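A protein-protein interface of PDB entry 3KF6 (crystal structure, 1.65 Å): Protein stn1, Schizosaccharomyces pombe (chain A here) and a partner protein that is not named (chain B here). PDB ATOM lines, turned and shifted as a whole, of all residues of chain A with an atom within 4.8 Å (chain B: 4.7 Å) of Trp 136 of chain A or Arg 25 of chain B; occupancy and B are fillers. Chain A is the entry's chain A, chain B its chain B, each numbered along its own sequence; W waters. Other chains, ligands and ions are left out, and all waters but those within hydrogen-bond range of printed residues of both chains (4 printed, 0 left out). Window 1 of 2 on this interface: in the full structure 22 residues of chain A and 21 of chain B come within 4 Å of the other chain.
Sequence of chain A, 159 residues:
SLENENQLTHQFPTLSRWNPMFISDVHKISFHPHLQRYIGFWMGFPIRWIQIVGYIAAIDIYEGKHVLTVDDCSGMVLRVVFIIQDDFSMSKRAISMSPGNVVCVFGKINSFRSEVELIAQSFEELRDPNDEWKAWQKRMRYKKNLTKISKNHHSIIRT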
ATOM      1  N   PHE A  22     -16.948 -10.390  32.611  1.00  0.00           N
ATOM      2  CA  PHE A  22     -17.501 -10.144  31.286  1.00  0.00           C
ATOM      3  C   PHE A  22     -19.007 -10.124  31.509  1.00  0.00           C
ATOM      4  O   PHE A  22     -19.525 -10.857  32.354  1.00  0.00           O
ATOM      5  CB  PHE A  22     -17.140 -11.270  30.316  1.00  0.00           C
ATOM      6  CG  PHE A  22     -15.742 -11.181  29.788  1.00  0.00           C
ATOM      7  CD1 PHE A  22     -14.830 -12.210  30.009  1.00  0.00           C
ATOM      8  CD2 PHE A  22     -15.332 -10.063  29.063  1.00  0.00           C
ATOM      9  CE1 PHE A  22     -13.526 -12.127  29.513  1.00  0.00           C
ATOM     10  CE2 PHE A  22     -14.029  -9.973  28.562  1.00  0.00           C
ATOM     11  CZ  PHE A  22     -13.127 -11.007  28.789  1.00  0.00           C
ATOM     12  N   TYR A  55     -18.205  -0.399  25.773  1.00  0.00           N
ATOM     13  CA  TYR A  55     -18.618   0.875  25.188  1.00  0.00           C
ATOM     14  C   TYR A  55     -20.111   1.096  25.418  1.00  0.00           C
ATOM     15  O   TYR A  55     -20.868   0.143  25.600  1.00  0.00           O
ATOM     16  CB  TYR A  55     -18.293   0.934  23.682  1.00  0.00           C
ATOM     17  CG  TYR A  55     -19.138   0.039  22.798  1.00  0.00           C
ATOM     18  CD1 TYR A  55     -18.746  -1.273  22.517  1.00  0.00           C
ATOM     19  CD2 TYR A  55     -20.350   0.493  22.273  1.00  0.00           C
ATOM     20  CE1 TYR A  55     -19.551  -2.118  21.736  1.00  0.00           C
ATOM     21  CE2 TYR A  55     -21.160  -0.343  21.493  1.00  0.00           C
ATOM     22  CZ  TYR A  55     -20.754  -1.644  21.235  1.00  0.00           C
ATOM     23  OH  TYR A  55     -21.581  -2.480  20.515  1.00  0.00           O
ATOM     24  N   ASP A  72     -19.651  -5.254  26.002  1.00  0.00           N
ATOM     25  CA  ASP A  72     -18.236  -5.620  26.040  1.00  0.00           C
ATOM     26  C   ASP A  72     -17.939  -6.723  25.013  1.00  0.00           C
ATOM     27  O   ASP A  72     -16.889  -7.363  25.059  1.00  0.00           O
ATOM     28  CB  ASP A  72     -17.824  -6.065  27.450  1.00  0.00           C
ATOM     29  CG  ASP A  72     -18.514  -7.332  27.890  1.00  0.00           C
ATOM     30  OD1 ASP A  72     -19.379  -7.827  27.137  1.00  0.00           O
ATOM     31  OD2 ASP A  72     -18.194  -7.832  28.996  1.00  0.00           O
ATOM     32  N   CYS A  73     -18.880  -6.916  24.086  1.00  0.00           N
ATOM     33  CA  CYS A  73     -18.775  -7.907  23.009  1.00  0.00           C
ATOM     34  C   CYS A  73     -18.794  -9.347  23.492  1.00  0.00           C
ATOM     35  O   CYS A  73     -18.437 -10.256  22.744  1.00  0.00           O
ATOM     36  CB  CYS A  73     -17.504  -7.680  22.180  1.00  0.00           C
ATOM     37  SG  CYS A  73     -17.401  -6.043  21.419  1.00  0.00           S
ATOM     38  N   GLU A 132      -8.916  -1.021  27.017  1.00  0.00           N
ATOM     39  CA  GLU A 132      -9.863  -2.104  26.796  1.00  0.00           C
ATOM     40  C   GLU A 132      -9.267  -3.497  26.680  1.00  0.00           C
ATOM     41  O   GLU A 132      -9.769  -4.424  27.312  1.00  0.00           O
ATOM     42  CB  GLU A 132     -10.746  -1.832  25.579  1.00  0.00           C
ATOM     43  CG  GLU A 132     -12.159  -1.459  25.964  1.00  0.00           C
ATOM     44  CD  GLU A 132     -13.107  -1.459  24.790  1.00  0.00           C
ATOM     45  OE1 GLU A 132     -12.805  -0.791  23.783  1.00  0.00           O
ATOM     46  OE2 GLU A 132     -14.160  -2.121  24.881  1.00  0.00           O
ATOM     47  N   TRP A 133      -8.213  -3.681  25.886  1.00  0.00           N
ATOM     48  CA  TRP A 133      -7.665  -5.024  25.808  1.00  0.00           C
ATOM     49  C   TRP A 133      -7.060  -5.442  27.142  1.00  0.00           C
ATOM     50  O   TRP A 133      -7.059  -6.625  27.470  1.00  0.00           O
ATOM     51  CB  TRP A 133      -6.648  -5.195  24.654  1.00  0.00           C
ATOM     52  CG  TRP A 133      -5.394  -4.383  24.728  1.00  0.00           C
ATOM     53  CD1 TRP A 133      -5.108  -3.261  24.006  1.00  0.00           C
ATOM     54  CD2 TRP A 133      -4.231  -4.656  25.526  1.00  0.00           C
ATOM     55  NE1 TRP A 133      -3.842  -2.819  24.298  1.00  0.00           N
ATOM     56  CE2 TRP A 133      -3.280  -3.654  25.228  1.00  0.00           C
ATOM     57  CE3 TRP A 133      -3.901  -5.649  26.462  1.00  0.00           C
ATOM     58  CZ2 TRP A 133      -2.016  -3.611  25.834  1.00  0.00           C
ATOM     59  CZ3 TRP A 133      -2.642  -5.609  27.067  1.00  0.00           C
ATOM     60  CH2 TRP A 133      -1.715  -4.594  26.746  1.00  0.00           C
ATOM     61  N   LYS A 134      -6.562  -4.481  27.920  1.00  0.00           N
ATOM     62  CA  LYS A 134      -6.006  -4.800  29.229  1.00  0.00           C
ATOM     63  C   LYS A 134      -7.151  -5.295  30.121  1.00  0.00           C
ATOM     64  O   LYS A 134      -6.972  -6.198  30.936  1.00  0.00           O
ATOM     65  CB  LYS A 134      -5.348  -3.565  29.858  1.00  0.00           C
ATOM     66  CG  LYS A 134      -4.031  -3.172  29.205  1.00  0.00           C
ATOM     67  CD  LYS A 134      -3.440  -1.916  29.833  1.00  0.00           C
ATOM     68  CE  LYS A 134      -2.074  -1.598  29.251  1.00  0.00           C
ATOM     69  NZ  LYS A 134      -1.488  -0.391  29.892  1.00  0.00           N
ATOM     70  N   ALA A 135      -8.332  -4.703  29.954  1.00  0.00           N
ATOM     71  CA  ALA A 135      -9.501  -5.104  30.736  1.00  0.00           C
ATOM     72  C   ALA A 135      -9.922  -6.518  30.343  1.00  0.00           C
ATOM     73  O   ALA A 135     -10.340  -7.312  31.192  1.00  0.00           O
ATOM     74  CB  ALA A 135     -10.648  -4.130  30.504  1.00  0.00           C
ATOM     75  N   TRP A 136      -9.814  -6.830  29.051  1.00  0.00           N
ATOM     76  CA  TRP A 136     -10.165  -8.164  28.580  1.00  0.00           C
ATOM     77  C   TRP A 136      -9.161  -9.170  29.132  1.00  0.00           C
ATOM     78  O   TRP A 136      -9.536 -10.264  29.547  1.00  0.00           O
ATOM     79  CB  TRP A 136     -10.166  -8.235  27.049  1.00  0.00           C
ATOM     80  CG  TRP A 136     -11.114  -7.281  26.395  1.00  0.00           C
ATOM     81  CD1 TRP A 136     -12.241  -6.731  26.940  1.00  0.00           C
ATOM     82  CD2 TRP A 136     -11.012  -6.757  25.070  1.00  0.00           C
ATOM     83  NE1 TRP A 136     -12.844  -5.889  26.035  1.00  0.00           N
ATOM     84  CE2 TRP A 136     -12.109  -5.887  24.878  1.00  0.00           C
ATOM     85  CE3 TRP A 136     -10.096  -6.933  24.023  1.00  0.00           C
ATOM     86  CZ2 TRP A 136     -12.315  -5.191  23.681  1.00  0.00           C
ATOM     87  CZ3 TRP A 136     -10.302  -6.240  22.832  1.00  0.00           C
ATOM     88  CH2 TRP A 136     -11.403  -5.380  22.675  1.00  0.00           C
ATOM     89  N   GLN A 137      -7.885  -8.787  29.132  1.00  0.00           N
ATOM     90  CA  GLN A 137      -6.817  -9.652  29.641  1.00  0.00           C
ATOM     91  C   GLN A 137      -7.079 -10.007  31.103  1.00  0.00           C
ATOM     92  O   GLN A 137      -7.040 -11.181  31.493  1.00  0.00           O
ATOM     93  CB  GLN A 137      -5.467  -8.940  29.518  1.00  0.00           C
ATOM     94  CG  GLN A 137      -4.303  -9.731  30.084  1.00  0.00           C
ATOM     95  CD  GLN A 137      -2.982  -9.022  29.890  1.00  0.00           C
ATOM     96  OE1 GLN A 137      -2.887  -7.804  30.052  1.00  0.00           O
ATOM     97  NE2 GLN A 137      -1.946  -9.784  29.555  1.00  0.00           N
ATOM     98  N   LYS A 138      -7.353  -8.984  31.904  1.00  0.00           N
ATOM     99  CA  LYS A 138      -7.628  -9.167  33.325  1.00  0.00           C
ATOM    100  C   LYS A 138      -8.803 -10.114  33.560  1.00  0.00           C
ATOM    101  O   LYS A 138      -8.761 -10.975  34.444  1.00  0.00           O
ATOM    102  CB  LYS A 138      -7.925  -7.813  33.972  1.00  0.00           C
ATOM    103  CG  LYS A 138      -8.311  -7.903  35.442  1.00  0.00           C
ATOM    104  CD  LYS A 138      -8.584  -6.530  36.040  1.00  0.00           C
ATOM    105  CE  LYS A 138      -7.329  -5.674  36.049  1.00  0.00           C
ATOM    106  NZ  LYS A 138      -7.558  -4.359  36.707  1.00  0.00           N
ATOM    107  N   ARG A 139      -9.860  -9.954  32.770  1.00  0.00           N
ATOM    108  CA  ARG A 139     -11.043 -10.794  32.918  1.00  0.00           C
ATOM    109  C   ARG A 139     -10.841 -12.253  32.526  1.00  0.00           C
ATOM    110  O   ARG A 139     -11.378 -13.150  33.172  1.00  0.00           O
ATOM    111  CB  ARG A 139     -12.207 -10.176  32.144  1.00  0.00           C
ATOM    112  CG  ARG A 139     -12.761  -8.979  32.897  1.00  0.00           C
ATOM    113  CD  ARG A 139     -13.577  -8.009  32.060  1.00  0.00           C
ATOM    114  NE  ARG A 139     -14.064  -6.956  32.945  1.00  0.00           N
ATOM    115  CZ  ARG A 139     -13.296  -6.024  33.506  1.00  0.00           C
ATOM    116  NH1 ARG A 139     -11.988  -5.979  33.260  1.00  0.00           N
ATOM    117  NH2 ARG A 139     -13.827  -5.172  34.375  1.00  0.00           N
ATOM    118  N   MET A 140     -10.068 -12.502  31.476  1.00  0.00           N
ATOM    119  CA  MET A 140      -9.835 -13.881  31.076  1.00  0.00           C
ATOM    120  C   MET A 140      -8.967 -14.588  32.117  1.00  0.00           C
ATOM    121  O   MET A 140      -9.191 -15.759  32.428  1.00  0.00           O
ATOM    122  CB  MET A 140      -9.192 -13.934  29.686  1.00  0.00           C
ATOM    123  CG  MET A 140     -10.163 -13.553  28.574  1.00  0.00           C
ATOM    124  SD  MET A 140      -9.458 -13.686  26.906  1.00  0.00           S
ATOM    125  CE  MET A 140      -8.498 -12.167  26.857  1.00  0.00           C
ATOM    126  N   ALA B   7     -22.078  -6.849  20.033  1.00  0.00           N
ATOM    127  CA  ALA B   7     -21.201  -6.986  18.880  1.00  0.00           C
ATOM    128  C   ALA B   7     -20.242  -8.170  19.000  1.00  0.00           C
ATOM    129  O   ALA B   7     -19.826  -8.549  20.103  1.00  0.00           O
ATOM    130  CB  ALA B   7     -20.409  -5.689  18.681  1.00  0.00           C
ATOM    131  N   LYS B   8     -19.925  -8.783  17.862  1.00  0.00           N
ATOM    132  CA  LYS B   8     -18.970  -9.887  17.827  1.00  0.00           C
ATOM    133  C   LYS B   8     -17.615  -9.259  17.544  1.00  0.00           C
ATOM    134  O   LYS B   8     -17.432  -8.606  16.513  1.00  0.00           O
ATOM    135  CB  LYS B   8     -19.304 -10.877  16.706  1.00  0.00           C
ATOM    136  CG  LYS B   8     -20.319 -11.933  17.091  1.00  0.00           C
ATOM    137  CD  LYS B   8     -20.650 -12.830  15.905  1.00  0.00           C
ATOM    138  CE  LYS B   8     -19.420 -13.531  15.342  1.00  0.00           C
ATOM    139  NZ  LYS B   8     -19.760 -14.296  14.099  1.00  0.00           N
ATOM    140  N   LEU B   9     -16.675  -9.446  18.462  1.00  0.00           N
ATOM    141  CA  LEU B   9     -15.331  -8.902  18.314  1.00  0.00           C
ATOM    142  C   LEU B   9     -14.533  -9.824  17.404  1.00  0.00           C
ATOM    143  O   LEU B   9     -14.241 -10.963  17.769  1.00  0.00           O
ATOM    144  CB  LEU B   9     -14.669  -8.796  19.689  1.00  0.00           C
ATOM    145  CG  LEU B   9     -13.263  -8.204  19.756  1.00  0.00           C
ATOM    146  CD1 LEU B   9     -13.273  -6.762  19.249  1.00  0.00           C
ATOM    147  CD2 LEU B   9     -12.778  -8.263  21.204  1.00  0.00           C
ATOM    148  N   ILE B  10     -14.167  -9.323  16.226  1.00  0.00           N
ATOM    149  CA  ILE B  10     -13.440 -10.133  15.249  1.00  0.00           C
ATOM    150  C   ILE B  10     -12.344  -9.369  14.511  1.00  0.00           C
ATOM    151  O   ILE B  10     -12.147  -8.179  14.721  1.00  0.00           O
ATOM    152  CB  ILE B  10     -14.397 -10.657  14.174  1.00  0.00           C
ATOM    153  CG1 ILE B  10     -15.035  -9.471  13.444  1.00  0.00           C
ATOM    154  CG2 ILE B  10     -15.474 -11.527  14.800  1.00  0.00           C
ATOM    155  CD1 ILE B  10     -15.874  -9.868  12.241  1.00  0.00           C
ATOM    156  N   LYS B  23     -24.071  -7.715  14.073  1.00  0.00           N
ATOM    157  CA  LYS B  23     -23.296  -6.568  14.547  1.00  0.00           C
ATOM    158  C   LYS B  23     -21.872  -7.037  14.807  1.00  0.00           C
ATOM    159  O   LYS B  23     -21.656  -8.033  15.489  1.00  0.00           O
ATOM    160  CB  LYS B  23     -23.891  -5.999  15.830  1.00  0.00           C
ATOM    161  CG  LYS B  23     -23.123  -4.787  16.364  1.00  0.00           C
ATOM    162  CD  LYS B  23     -23.746  -4.235  17.643  1.00  0.00           C
ATOM    163  CE  LYS B  23     -25.134  -3.666  17.402  1.00  0.00           C
ATOM    164  NZ  LYS B  23     -25.759  -3.151  18.656  1.00  0.00           N
ATOM    165  N   LEU B  24     -20.900  -6.296  14.278  1.00  0.00           N
ATOM    166  CA  LEU B  24     -19.497  -6.669  14.412  1.00  0.00           C
ATOM    167  C   LEU B  24     -18.641  -5.519  14.920  1.00  0.00           C
ATOM    168  O   LEU B  24     -18.941  -4.359  14.664  1.00  0.00           O
ATOM    169  CB  LEU B  24     -18.938  -7.084  13.048  1.00  0.00           C
ATOM    170  CG  LEU B  24     -19.743  -8.068  12.198  1.00  0.00           C
ATOM    171  CD1 LEU B  24     -19.140  -8.144  10.793  1.00  0.00           C
ATOM    172  CD2 LEU B  24     -19.740  -9.432  12.869  1.00  0.00           C
ATOM    173  N   ARG B  25     -17.580  -5.850  15.643  1.00  0.00           N
ATOM    174  CA  ARG B  25     -16.644  -4.831  16.099  1.00  0.00           C
ATOM    175  C   ARG B  25     -15.255  -5.261  15.643  1.00  0.00           C
ATOM    176  O   ARG B  25     -14.841  -6.399  15.877  1.00  0.00           O
ATOM    177  CB  ARG B  25     -16.655  -4.660  17.622  1.00  0.00           C
ATOM    178  CG  ARG B  25     -15.528  -3.726  18.053  1.00  0.00           C
ATOM    179  CD  ARG B  25     -15.425  -3.529  19.546  1.00  0.00           C
ATOM    180  NE  ARG B  25     -14.137  -2.929  19.890  1.00  0.00           N
ATOM    181  CZ  ARG B  25     -13.838  -2.439  21.089  1.00  0.00           C
ATOM    182  NH1 ARG B  25     -14.738  -2.471  22.068  1.00  0.00           N
ATOM    183  NH2 ARG B  25     -12.637  -1.920  21.310  1.00  0.00           N
ATOM    184  N   PHE B  26     -14.539  -4.356  14.981  1.00  0.00           N
ATOM    185  CA  PHE B  26     -13.202  -4.668  14.500  1.00  0.00           C
ATOM    186  C   PHE B  26     -12.341  -3.423  14.350  1.00  0.00           C
ATOM    187  O   PHE B  26     -12.847  -2.296  14.322  1.00  0.00           O
ATOM    188  CB  PHE B  26     -13.273  -5.408  13.155  1.00  0.00           C
ATOM    189  CG  PHE B  26     -14.068  -4.688  12.105  1.00  0.00           C
ATOM    190  CD1 PHE B  26     -15.438  -4.876  12.002  1.00  0.00           C
ATOM    191  CD2 PHE B  26     -13.442  -3.809  11.224  1.00  0.00           C
ATOM    192  CE1 PHE B  26     -16.184  -4.198  11.032  1.00  0.00           C
ATOM    193  CE2 PHE B  26     -14.178  -3.124  10.255  1.00  0.00           C
ATOM    194  CZ  PHE B  26     -15.548  -3.320  10.162  1.00  0.00           C
ATOM    195  N   ASN B  67     -11.478   2.031  15.284  1.00  0.00           N
ATOM    196  CA  ASN B  67     -12.297   0.964  15.864  1.00  0.00           C
ATOM    197  C   ASN B  67     -13.663   1.169  15.219  1.00  0.00           C
ATOM    198  O   ASN B  67     -14.169   2.292  15.166  1.00  0.00           O
ATOM    199  CB  ASN B  67     -12.432   1.102  17.383  1.00  0.00           C
ATOM    200  CG  ASN B  67     -11.251   0.531  18.132  1.00  0.00           C
ATOM    201  OD1 ASN B  67     -10.780  -0.570  17.837  1.00  0.00           O
ATOM    202  ND2 ASN B  67     -10.772   1.270  19.123  1.00  0.00           N
ATOM    203  N   ILE B  68     -14.262   0.084  14.746  1.00  0.00           N
ATOM    204  CA  ILE B  68     -15.547   0.146  14.068  1.00  0.00           C
ATOM    205  C   ILE B  68     -16.578  -0.789  14.678  1.00  0.00           C
ATOM    206  O   ILE B  68     -16.261  -1.920  15.020  1.00  0.00           O
ATOM    207  CB  ILE B  68     -15.404  -0.288  12.577  1.00  0.00           C
ATOM    208  CG1 ILE B  68     -14.475   0.669  11.828  1.00  0.00           C
ATOM    209  CG2 ILE B  68     -16.773  -0.343  11.899  1.00  0.00           C
ATOM    210  CD1 ILE B  68     -15.026   2.061  11.671  1.00  0.00           C
ATOM    211  N   VAL B  69     -17.800  -0.292  14.835  1.00  0.00           N
ATOM    212  CA  VAL B  69     -18.911  -1.125  15.275  1.00  0.00           C
ATOM    213  C   VAL B  69     -19.922  -0.910  14.161  1.00  0.00           C
ATOM    214  O   VAL B  69     -20.255   0.229  13.835  1.00  0.00           O
ATOM    215  CB  VAL B  69     -19.541  -0.683  16.606  1.00  0.00           C
ATOM    216  CG1 VAL B  69     -20.796  -1.534  16.878  1.00  0.00           C
ATOM    217  CG2 VAL B  69     -18.549  -0.864  17.737  1.00  0.00           C
ATOM    218  N   TYR B  94      -3.446  -6.170  21.282  1.00  0.00           N
ATOM    219  CA  TYR B  94      -4.851  -6.165  20.895  1.00  0.00           C
ATOM    220  C   TYR B  94      -5.228  -7.442  20.135  1.00  0.00           C
ATOM    221  O   TYR B  94      -6.236  -8.082  20.446  1.00  0.00           O
ATOM    222  CB  TYR B  94      -5.166  -4.938  20.033  1.00  0.00           C
ATOM    223  CG  TYR B  94      -6.514  -5.006  19.350  1.00  0.00           C
ATOM    224  CD1 TYR B  94      -6.637  -5.532  18.066  1.00  0.00           C
ATOM    225  CD2 TYR B  94      -7.674  -4.591  20.003  1.00  0.00           C
ATOM    226  CE1 TYR B  94      -7.874  -5.646  17.448  1.00  0.00           C
ATOM    227  CE2 TYR B  94      -8.923  -4.700  19.391  1.00  0.00           C
ATOM    228  CZ  TYR B  94      -9.011  -5.230  18.113  1.00  0.00           C
ATOM    229  OH  TYR B  94     -10.238  -5.349  17.503  1.00  0.00           O
ATOM    230  N   MET B  97      -5.396 -10.489  22.471  1.00  0.00           N
ATOM    231  CA  MET B  97      -6.612 -10.580  23.271  1.00  0.00           C
ATOM    232  C   MET B  97      -7.862 -10.907  22.460  1.00  0.00           C
ATOM    233  O   MET B  97      -8.756 -11.586  22.959  1.00  0.00           O
ATOM    234  CB  MET B  97      -6.834  -9.295  24.074  1.00  0.00           C
ATOM    235  CG  MET B  97      -5.710  -8.971  25.053  1.00  0.00           C
ATOM    236  SD  MET B  97      -5.141 -10.389  26.037  1.00  0.00           S
ATOM    237  CE  MET B  97      -3.431  -9.902  26.338  1.00  0.00           C
ATOM    238  N   VAL B  98      -7.945 -10.419  21.222  1.00  0.00           N
ATOM    239  CA  VAL B  98      -9.102 -10.722  20.389  1.00  0.00           C
ATOM    240  C   VAL B  98      -9.107 -12.227  20.146  1.00  0.00           C
ATOM    241  O   VAL B  98     -10.148 -12.871  20.218  1.00  0.00           O
ATOM    242  CB  VAL B  98      -9.051 -10.009  19.013  1.00  0.00           C
ATOM    243  CG1 VAL B  98     -10.143 -10.560  18.097  1.00  0.00           C
ATOM    244  CG2 VAL B  98      -9.238  -8.515  19.195  1.00  0.00           C
ATOM    245  N   ARG B 101     -10.031 -14.165  23.396  1.00  0.00           N
ATOM    246  CA  ARG B 101     -11.455 -14.098  23.697  1.00  0.00           C
ATOM    247  C   ARG B 101     -12.278 -15.046  22.837  1.00  0.00           C
ATOM    248  O   ARG B 101     -13.316 -15.532  23.270  1.00  0.00           O
ATOM    249  CB  ARG B 101     -11.982 -12.670  23.529  1.00  0.00           C
ATOM    250  CG  ARG B 101     -11.489 -11.733  24.601  1.00  0.00           C
ATOM    251  CD  ARG B 101     -12.292 -10.464  24.617  1.00  0.00           C
ATOM    252  NE  ARG B 101     -13.714 -10.723  24.847  1.00  0.00           N
ATOM    253  CZ  ARG B 101     -14.627  -9.764  24.964  1.00  0.00           C
ATOM    254  NH1 ARG B 101     -14.264  -8.492  24.877  1.00  0.00           N
ATOM    255  NH2 ARG B 101     -15.906 -10.076  25.146  1.00  0.00           N
HETATM  256  O   HOH W   1     -16.712  -3.565  23.735  1.00  0.00           O
HETATM  257  O   HOH W   2     -20.996 -11.025  20.741  1.00  0.00           O
HETATM  258  O   HOH W   3     -17.080 -11.199  20.620  1.00  0.00           O
HETATM  259  O   HOH W   4     -24.179  -1.595  20.206  1.00  0.00           O
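NH2 of Arg 101 of chain B sits close to O of Cys 73 of chain A (3.5 Å). The guanidinium group of Arg 101 of chain B sits close to the indole nitrogen of Trp 136 of chain A, 3.2 Å away. OE1 of Glu 132 of chain A is in salt-bridge range of NH2 of Arg 25 of chain B. The side-chain sulfur (SG) of Cys 73 of chain A lies close to the backbone carbonyl oxygen (O) of Ala 7 of chain B (3.7 Å). SD of Met 140 of chain A sits at hydrogen-bond distance from N of Arg 101 of chain B (3.6 Å). The backbone carbonyl oxygen (O) of Asp 72 of chain A sits at hydrogen-bond distance from the guanidinium group (NH1) of Arg 101 of chain B, 2.9 Å away.
O of Lys 8 of chain B sits at hydrogen-bond distance from N of Arg 25 of chain B (2.9 Å). The backbone NH (N) of Ile 10 of chain B is in hydrogen-bond range of the backbone carbonyl oxygen (O) of Arg 25 of chain B (3.0 Å).
Phe 22 of chain A touches Arg 101 of chain B. Ala 7 of chain B touches Tyr 55 of chain A. Tyr 55 of chain A touches Val 69 of chain B (OH to CG1, 3.8 Å). Cys 73 of chain A touches Leu 9 of chain B (CB to CB, 3.9 Å). Arg 25 of chain B touches Cys 73 of chain A (CD to SG, 3.7 Å). Trp 133 of chain A touches Met 97 of chain B (O to CG, 3.6 Å). CD2 of Leu 9 of chain B touches CH2 of Trp 136 of chain A (3.5 Å). Trp 136 of chain A touches Arg 25 of chain B. NE2 of Gln 137 of chain A touches CE of Met 97 of chain B, at 3.5 Å. Met 140 of chain A touches Met 97 of chain B.
Printed residues of chain B within 4 Å of Trp 136 of chain A: Leu 9, Arg 25 and Arg 101. Arg 25 of chain B touches just these residues of chain A: Cys 73 (3.7 Å), Glu 132 (2.7 Å) and Trp 136 (3.9 Å). Of the printed residues of chain A, Val 69 of chain B touches Tyr 55. Of the printed residues of chain B, Cys 73 of chain A touches Ala 7, Leu 9, Arg 25 and Arg 101. Of the printed residues of chain A, Arg 101 of chain B touches Phe 22 (3.7 Å), Asp 72 (2.9 Å), Cys 73 (3.4 Å), Trp 136 (3.2 Å) and Met 140 (3.6 Å). Of the printed residues of chain A, Leu 9 of chain B touches Cys 73 and Trp 136. Printed residues of chain A within 4 Å of Ala 7 of chain B: Tyr 55 and Cys 73. The nearest printed residue of chain B that does not touch Trp 136 of chain A is Tyr 94 of chain B (4.01 Å). The nearest printed residue of chain A that does not touch Val 69 of chain B is Cys 73 of chain A (6.5 Å).
Printed residues of chain A that touch a printed residue of chain B: Phe 22, Tyr 55, Asp 72, Cys 73, Glu 132, Trp 133, Trp 136, Gln 137 and Met 140. Hydrophobic or aromatic side chains of chain A that line the printed part of chain B: Phe 22, Tyr 55, Trp 133, Trp 136 and Met 140. Among the printed residues, 16 pairs touch across the chains. Among the printed residues, Asp or Glu carboxylates within 4 Å of a Lys or Arg side-chain nitrogen of the other chain: Glu 132 of chain A with Arg 25 of chain B (2.7 Å).
Water W3 bridges the backbone carbonyl oxygen (O) of Cys 73 of chain A (2.7 Å) and the backbone NH (N) of Leu 9 of chain B (2.8 Å). Water W4 lies within hydrogen-bond range of the side-chain amino group (NZ) of Lys 23 of chain B (2.7 Å) and the side-chain hydroxyl (OH) of Tyr 55 of chain A (2.8 Å). Water W1 lies within hydrogen-bond range of the guanidinium group (NH1) of Arg 25 of chain B (2.8 Å), the side-chain carboxylate (OE2) of Glu 132 of chain A (3.1 Å) and the side-chain sulfur (SG) of Cys 73 of chain A (3.5 Å). Water W2 bridges O of Ala 7 of chain B (2.8 Å) and O of Cys 73 of chain A (3.3 Å).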
